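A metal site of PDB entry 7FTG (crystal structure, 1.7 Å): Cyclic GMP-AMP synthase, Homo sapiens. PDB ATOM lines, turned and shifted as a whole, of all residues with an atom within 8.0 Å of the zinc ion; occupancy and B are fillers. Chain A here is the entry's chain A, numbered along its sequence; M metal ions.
N of Cys 237 is in hydrogen-bond range of O of Glu 242.
A ring nitrogen (ND1) of His 230 lies within hydrogen-bond range of the backbone carbonyl oxygen of Leu 227 (2.9 Å).
O of His 230 lies within hydrogen-bond range of NE of Arg 246, 3.4 Å away.
O of Cys 244 is in hydrogen-bond range of NH2 of Arg 297.
The guanidinium group (NH2) of Arg 246 sits close to the side-chain sulfur (SG) of Cys 236, at 3.7 Å.
SG of Cys 244 sits close to NH2 of Arg 246 (3.4 Å).
Within 4 Å of the zinc ion: His 230, Cys 236, Cys 237 and Cys 244.
The zinc ion is bound by NE2 of His 230 (2.1 Å), SG of Cys 237 (2.4 Å), SG of Cys 236 (2.4 Å) and SG of Cys 244 (2.4 Å).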
ATOM      1  N   LEU A 227       4.808 -17.505  19.031  1.00  0.00           N
ATOM      2  CA  LEU A 227       5.775 -18.197  18.181  1.00  0.00           C
ATOM      3  C   LEU A 227       5.191 -18.487  16.812  1.00  0.00           C
ATOM      4  O   LEU A 227       5.900 -18.440  15.795  1.00  0.00           O
ATOM      5  CB  LEU A 227       6.205 -19.520  18.856  1.00  0.00           C
ATOM      6  CG  LEU A 227       7.220 -19.400  19.978  1.00  0.00           C
ATOM      7  CD1 LEU A 227       7.366 -20.734  20.691  1.00  0.00           C
ATOM      8  CD2 LEU A 227       8.547 -18.962  19.363  1.00  0.00           C
ATOM      9  N   ASN A 228       3.902 -18.836  16.757  1.00  0.00           N
ATOM     10  CA  ASN A 228       3.306 -19.209  15.489  1.00  0.00           C
ATOM     11  C   ASN A 228       2.820 -18.009  14.689  1.00  0.00           C
ATOM     12  O   ASN A 228       2.688 -18.103  13.471  1.00  0.00           O
ATOM     13  CB  ASN A 228       2.133 -20.167  15.711  1.00  0.00           C
ATOM     14  CG  ASN A 228       2.595 -21.576  16.044  1.00  0.00           C
ATOM     15  OD1 ASN A 228       3.697 -21.976  15.687  1.00  0.00           O
ATOM     16  ND2 ASN A 228       1.737 -22.336  16.705  1.00  0.00           N
ATOM     17  N   ASN A 229       2.532 -16.902  15.357  1.00  0.00           N
ATOM     18  CA  ASN A 229       2.043 -15.684  14.707  1.00  0.00           C
ATOM     19  C   ASN A 229       3.021 -14.581  15.108  1.00  0.00           C
ATOM     20  O   ASN A 229       2.746 -13.781  15.997  1.00  0.00           O
ATOM     21  CB  ASN A 229       0.607 -15.384  15.169  1.00  0.00           C
ATOM     22  CG  ASN A 229      -0.056 -14.312  14.334  1.00  0.00           C
ATOM     23  OD1 ASN A 229       0.539 -13.751  13.419  1.00  0.00           O
ATOM     24  ND2 ASN A 229      -1.331 -14.027  14.652  1.00  0.00           N
ATOM     25  N   HIS A 230       4.205 -14.625  14.492  1.00  0.00           N
ATOM     26  CA  HIS A 230       5.420 -14.069  15.101  1.00  0.00           C
ATOM     27  C   HIS A 230       5.961 -12.850  14.384  1.00  0.00           C
ATOM     28  O   HIS A 230       7.011 -12.344  14.781  1.00  0.00           O
ATOM     29  CB  HIS A 230       6.514 -15.133  15.141  1.00  0.00           C
ATOM     30  CG  HIS A 230       6.868 -15.650  13.775  1.00  0.00           C
ATOM     31  ND1 HIS A 230       6.704 -16.969  13.407  1.00  0.00           N
ATOM     32  CD2 HIS A 230       7.302 -14.989  12.675  1.00  0.00           C
ATOM     33  CE1 HIS A 230       7.081 -17.107  12.150  1.00  0.00           C
ATOM     34  NE2 HIS A 230       7.416 -15.925  11.676  1.00  0.00           N
ATOM     35  N   GLY A 231       5.358 -12.441  13.284  1.00  0.00           N
ATOM     36  CA  GLY A 231       5.907 -11.376  12.484  1.00  0.00           C
ATOM     37  C   GLY A 231       5.305 -10.017  12.808  1.00  0.00           C
ATOM     38  O   GLY A 231       4.205  -9.904  13.368  1.00  0.00           O
ATOM     39  N   LYS A 232       6.025  -8.950  12.441  1.00  0.00           N
ATOM     40  CA  LYS A 232       5.383  -7.655  12.400  1.00  0.00           C
ATOM     41  C   LYS A 232       4.323  -7.628  11.327  1.00  0.00           C
ATOM     42  O   LYS A 232       3.200  -7.139  11.544  1.00  0.00           O
ATOM     43  CB  LYS A 232       6.397  -6.532  12.148  1.00  0.00           C
ATOM     44  CG  LYS A 232       5.663  -5.185  12.010  1.00  0.00           C
ATOM     45  CD  LYS A 232       6.627  -3.989  11.978  1.00  0.00           C
ATOM     46  CE  LYS A 232       7.343  -3.831  13.332  1.00  0.00           C
ATOM     47  NZ  LYS A 232       6.363  -3.652  14.486  1.00  0.00           N
ATOM     48  N   SER A 233       4.660  -8.173  10.151  1.00  0.00           N
ATOM     49  CA  SER A 233       3.684  -8.366   9.079  1.00  0.00           C
ATOM     50  C   SER A 233       2.747  -9.505   9.436  1.00  0.00           C
ATOM     51  O   SER A 233       3.188 -10.584   9.876  1.00  0.00           O
ATOM     52  CB  SER A 233       4.414  -8.684   7.771  1.00  0.00           C
ATOM     53  OG  SER A 233       3.477  -9.017   6.754  1.00  0.00           O
ATOM     54  N   THR A 235       1.407 -11.275   7.338  1.00  0.00           N
ATOM     55  CA  THR A 235       1.704 -12.331   6.361  1.00  0.00           C
ATOM     56  C   THR A 235       3.136 -12.845   6.452  1.00  0.00           C
ATOM     57  O   THR A 235       3.612 -13.522   5.517  1.00  0.00           O
ATOM     58  CB  THR A 235       1.369 -11.882   4.922  1.00  0.00           C
ATOM     59  OG1 THR A 235       1.868 -10.565   4.667  1.00  0.00           O
ATOM     60  CG2 THR A 235      -0.160 -11.869   4.698  1.00  0.00           C
ATOM     61  N   CYS A 236       3.831 -12.582   7.553  1.00  0.00           N
ATOM     62  CA  CYS A 236       5.143 -13.182   7.764  1.00  0.00           C
ATOM     63  C   CYS A 236       5.053 -14.697   7.615  1.00  0.00           C
ATOM     64  O   CYS A 236       4.184 -15.346   8.202  1.00  0.00           O
ATOM     65  CB  CYS A 236       5.681 -12.814   9.150  1.00  0.00           C
ATOM     66  SG  CYS A 236       7.514 -13.079   9.313  1.00  0.00           S
ATOM     67  N   CYS A 237       5.944 -15.248   6.788  1.00  0.00           N
ATOM     68  CA  CYS A 237       6.041 -16.680   6.495  1.00  0.00           C
ATOM     69  C   CYS A 237       4.805 -17.255   5.791  1.00  0.00           C
ATOM     70  O   CYS A 237       4.656 -18.480   5.705  1.00  0.00           O
ATOM     71  CB  CYS A 237       6.382 -17.471   7.764  1.00  0.00           C
ATOM     72  SG  CYS A 237       8.124 -17.164   8.296  1.00  0.00           S
ATOM     73  N   GLU A 238       3.929 -16.419   5.241  1.00  0.00           N
ATOM     74  CA  GLU A 238       2.821 -16.909   4.424  1.00  0.00           C
ATOM     75  C   GLU A 238       3.095 -16.824   2.930  1.00  0.00           C
ATOM     76  O   GLU A 238       2.231 -17.223   2.138  1.00  0.00           O
ATOM     77  CB  GLU A 238       1.517 -16.152   4.747  1.00  0.00           C
ATOM     78  CG  GLU A 238       0.996 -16.494   6.129  1.00  0.00           C
ATOM     79  CD  GLU A 238      -0.452 -16.038   6.366  1.00  0.00           C
ATOM     80  OE1 GLU A 238      -1.058 -15.401   5.466  1.00  0.00           O
ATOM     81  OE2 GLU A 238      -0.976 -16.346   7.449  1.00  0.00           O
ATOM     82  N   ASN A 239       4.256 -16.341   2.510  1.00  0.00           N
ATOM     83  CA  ASN A 239       4.607 -16.256   1.096  1.00  0.00           C
ATOM     84  C   ASN A 239       6.121 -16.216   0.965  1.00  0.00           C
ATOM     85  O   ASN A 239       6.838 -15.926   1.936  1.00  0.00           O
ATOM     86  CB  ASN A 239       4.000 -15.006   0.444  1.00  0.00           C
ATOM     87  CG  ASN A 239       4.460 -13.724   1.094  1.00  0.00           C
ATOM     88  OD1 ASN A 239       5.600 -13.301   0.905  1.00  0.00           O
ATOM     89  ND2 ASN A 239       3.570 -13.066   1.839  1.00  0.00           N
ATOM     90  N   GLU A 242       8.264 -13.198   2.187  1.00  0.00           N
ATOM     91  CA  GLU A 242       8.280 -12.880   3.615  1.00  0.00           C
ATOM     92  C   GLU A 242       8.702 -14.068   4.450  1.00  0.00           C
ATOM     93  O   GLU A 242       8.064 -14.431   5.434  1.00  0.00           O
ATOM     94  CB  GLU A 242       6.908 -12.386   4.105  1.00  0.00           C
ATOM     95  CG  GLU A 242       6.510 -11.050   3.480  1.00  0.00           C
ATOM     96  CD  GLU A 242       5.187 -10.523   4.056  1.00  0.00           C
ATOM     97  OE1 GLU A 242       5.205 -10.062   5.198  1.00  0.00           O
ATOM     98  OE2 GLU A 242       4.144 -10.584   3.350  1.00  0.00           O
ATOM     99  N   LYS A 243       9.839 -14.667   4.117  1.00  0.00           N
ATOM    100  CA  LYS A 243      10.321 -15.840   4.844  1.00  0.00           C
ATOM    101  C   LYS A 243      11.344 -15.364   5.862  1.00  0.00           C
ATOM    102  O   LYS A 243      12.459 -14.962   5.481  1.00  0.00           O
ATOM    103  CB  LYS A 243      10.927 -16.878   3.885  1.00  0.00           C
ATOM    104  CG  LYS A 243       9.980 -17.386   2.800  1.00  0.00           C
ATOM    105  CD  LYS A 243       8.719 -18.023   3.391  1.00  0.00           C
ATOM    106  CE  LYS A 243       9.014 -19.359   4.080  1.00  0.00           C
ATOM    107  NZ  LYS A 243       7.836 -19.855   4.863  1.00  0.00           N
ATOM    108  N   CYS A 244      10.980 -15.377   7.131  1.00  0.00           N
ATOM    109  CA  CYS A 244      11.890 -14.965   8.188  1.00  0.00           C
ATOM    110  C   CYS A 244      12.531 -16.198   8.826  1.00  0.00           C
ATOM    111  O   CYS A 244      12.129 -17.330   8.573  1.00  0.00           O
ATOM    112  CB  CYS A 244      11.167 -14.110   9.220  1.00  0.00           C
ATOM    113  SG  CYS A 244      10.329 -14.989  10.535  1.00  0.00           S
ATOM    114  N   CYS A 245      13.577 -15.986   9.644  1.00  0.00           N
ATOM    115  CA  CYS A 245      14.283 -17.091  10.262  1.00  0.00           C
ATOM    116  C   CYS A 245      14.094 -17.147  11.779  1.00  0.00           C
ATOM    117  O   CYS A 245      14.912 -17.744  12.482  1.00  0.00           O
ATOM    118  CB  CYS A 245      15.784 -17.052   9.917  1.00  0.00           C
ATOM    119  SG  CYS A 245      16.629 -15.605  10.557  1.00  0.00           S
ATOM    120  N   ARG A 246      12.997 -16.607  12.298  1.00  0.00           N
ATOM    121  CA  ARG A 246      12.804 -16.595  13.751  1.00  0.00           C
ATOM    122  C   ARG A 246      12.699 -18.005  14.318  1.00  0.00           C
ATOM    123  O   ARG A 246      13.354 -18.340  15.325  1.00  0.00           O
ATOM    124  CB  ARG A 246      11.560 -15.792  14.113  1.00  0.00           C
ATOM    125  CG  ARG A 246      11.736 -14.284  14.011  1.00  0.00           C
ATOM    126  CD  ARG A 246      10.414 -13.611  14.427  1.00  0.00           C
ATOM    127  NE  ARG A 246      10.355 -12.153  14.379  1.00  0.00           N
ATOM    128  CZ  ARG A 246       9.930 -11.455  13.328  1.00  0.00           C
ATOM    129  NH1 ARG A 246       9.817 -10.139  13.428  1.00  0.00           N
ATOM    130  NH2 ARG A 246       9.645 -12.085  12.182  1.00  0.00           N
ATOM    131  N   LYS A 247      11.827 -18.838  13.734  1.00  0.00           N
ATOM    132  CA  LYS A 247      11.673 -20.186  14.284  1.00  0.00           C
ATOM    133  C   LYS A 247      12.975 -20.979  14.165  1.00  0.00           C
ATOM    134  O   LYS A 247      13.325 -21.740  15.075  1.00  0.00           O
ATOM    135  CB  LYS A 247      10.544 -20.941  13.586  1.00  0.00           C
ATOM    136  CG  LYS A 247       9.145 -20.425  13.932  1.00  0.00           C
ATOM    137  CD  LYS A 247       8.086 -21.420  13.399  1.00  0.00           C
ATOM    138  CE  LYS A 247       6.698 -21.072  13.922  1.00  0.00           C
ATOM    139  NZ  LYS A 247       5.630 -21.946  13.324  1.00  0.00           N
ATOM    140  N   ASP A 292      10.552  -7.400  10.699  1.00  0.00           N
ATOM    141  CA  ASP A 292      10.802  -8.654   9.981  1.00  0.00           C
ATOM    142  C   ASP A 292      12.094  -8.559   9.177  1.00  0.00           C
ATOM    143  O   ASP A 292      12.750  -9.580   8.954  1.00  0.00           O
ATOM    144  CB  ASP A 292       9.639  -9.020   9.060  1.00  0.00           C
ATOM    145  CG  ASP A 292       8.331  -9.176   9.818  1.00  0.00           C
ATOM    146  OD1 ASP A 292       8.402  -9.445  11.030  1.00  0.00           O
ATOM    147  OD2 ASP A 292       7.254  -9.048   9.188  1.00  0.00           O
ATOM    148  N   TRP A 295      15.107 -10.305  10.504  1.00  0.00           N
ATOM    149  CA  TRP A 295      15.066 -11.756  10.589  1.00  0.00           C
ATOM    150  C   TRP A 295      14.991 -12.359   9.198  1.00  0.00           C
ATOM    151  O   TRP A 295      14.398 -13.436   9.009  1.00  0.00           O
ATOM    152  CB  TRP A 295      13.865 -12.198  11.435  1.00  0.00           C
ATOM    153  CG  TRP A 295      13.930 -11.718  12.866  1.00  0.00           C
ATOM    154  CD1 TRP A 295      13.395 -10.562  13.378  1.00  0.00           C
ATOM    155  CD2 TRP A 295      14.586 -12.376  13.942  1.00  0.00           C
ATOM    156  NE1 TRP A 295      13.665 -10.478  14.731  1.00  0.00           N
ATOM    157  CE2 TRP A 295      14.401 -11.581  15.103  1.00  0.00           C
ATOM    158  CE3 TRP A 295      15.306 -13.577  14.045  1.00  0.00           C
ATOM    159  CZ2 TRP A 295      14.900 -11.944  16.352  1.00  0.00           C
ATOM    160  CZ3 TRP A 295      15.803 -13.950  15.284  1.00  0.00           C
ATOM    161  CH2 TRP A 295      15.585 -13.142  16.430  1.00  0.00           C
ATOM    162  N   ARG A 297      15.622 -14.522   6.134  1.00  0.00           N
ATOM    163  CA  ARG A 297      16.201 -15.863   6.026  1.00  0.00           C
ATOM    164  C   ARG A 297      17.635 -15.837   5.531  1.00  0.00           C
ATOM    165  O   ARG A 297      18.468 -16.641   5.961  1.00  0.00           O
ATOM    166  CB  ARG A 297      15.333 -16.711   5.078  1.00  0.00           C
ATOM    167  CG  ARG A 297      15.970 -18.016   4.625  1.00  0.00           C
ATOM    168  CD  ARG A 297      14.910 -19.066   4.282  1.00  0.00           C
ATOM    169  NE  ARG A 297      13.878 -19.133   5.315  1.00  0.00           N
ATOM    170  CZ  ARG A 297      14.050 -19.690   6.520  1.00  0.00           C
ATOM    171  NH1 ARG A 297      15.215 -20.223   6.861  1.00  0.00           N
ATOM    172  NH2 ARG A 297      13.046 -19.710   7.393  1.00  0.00           N
HETATM  173 ZN    ZN M   1       8.100 -15.327   9.782  1.00  0.00          ZN
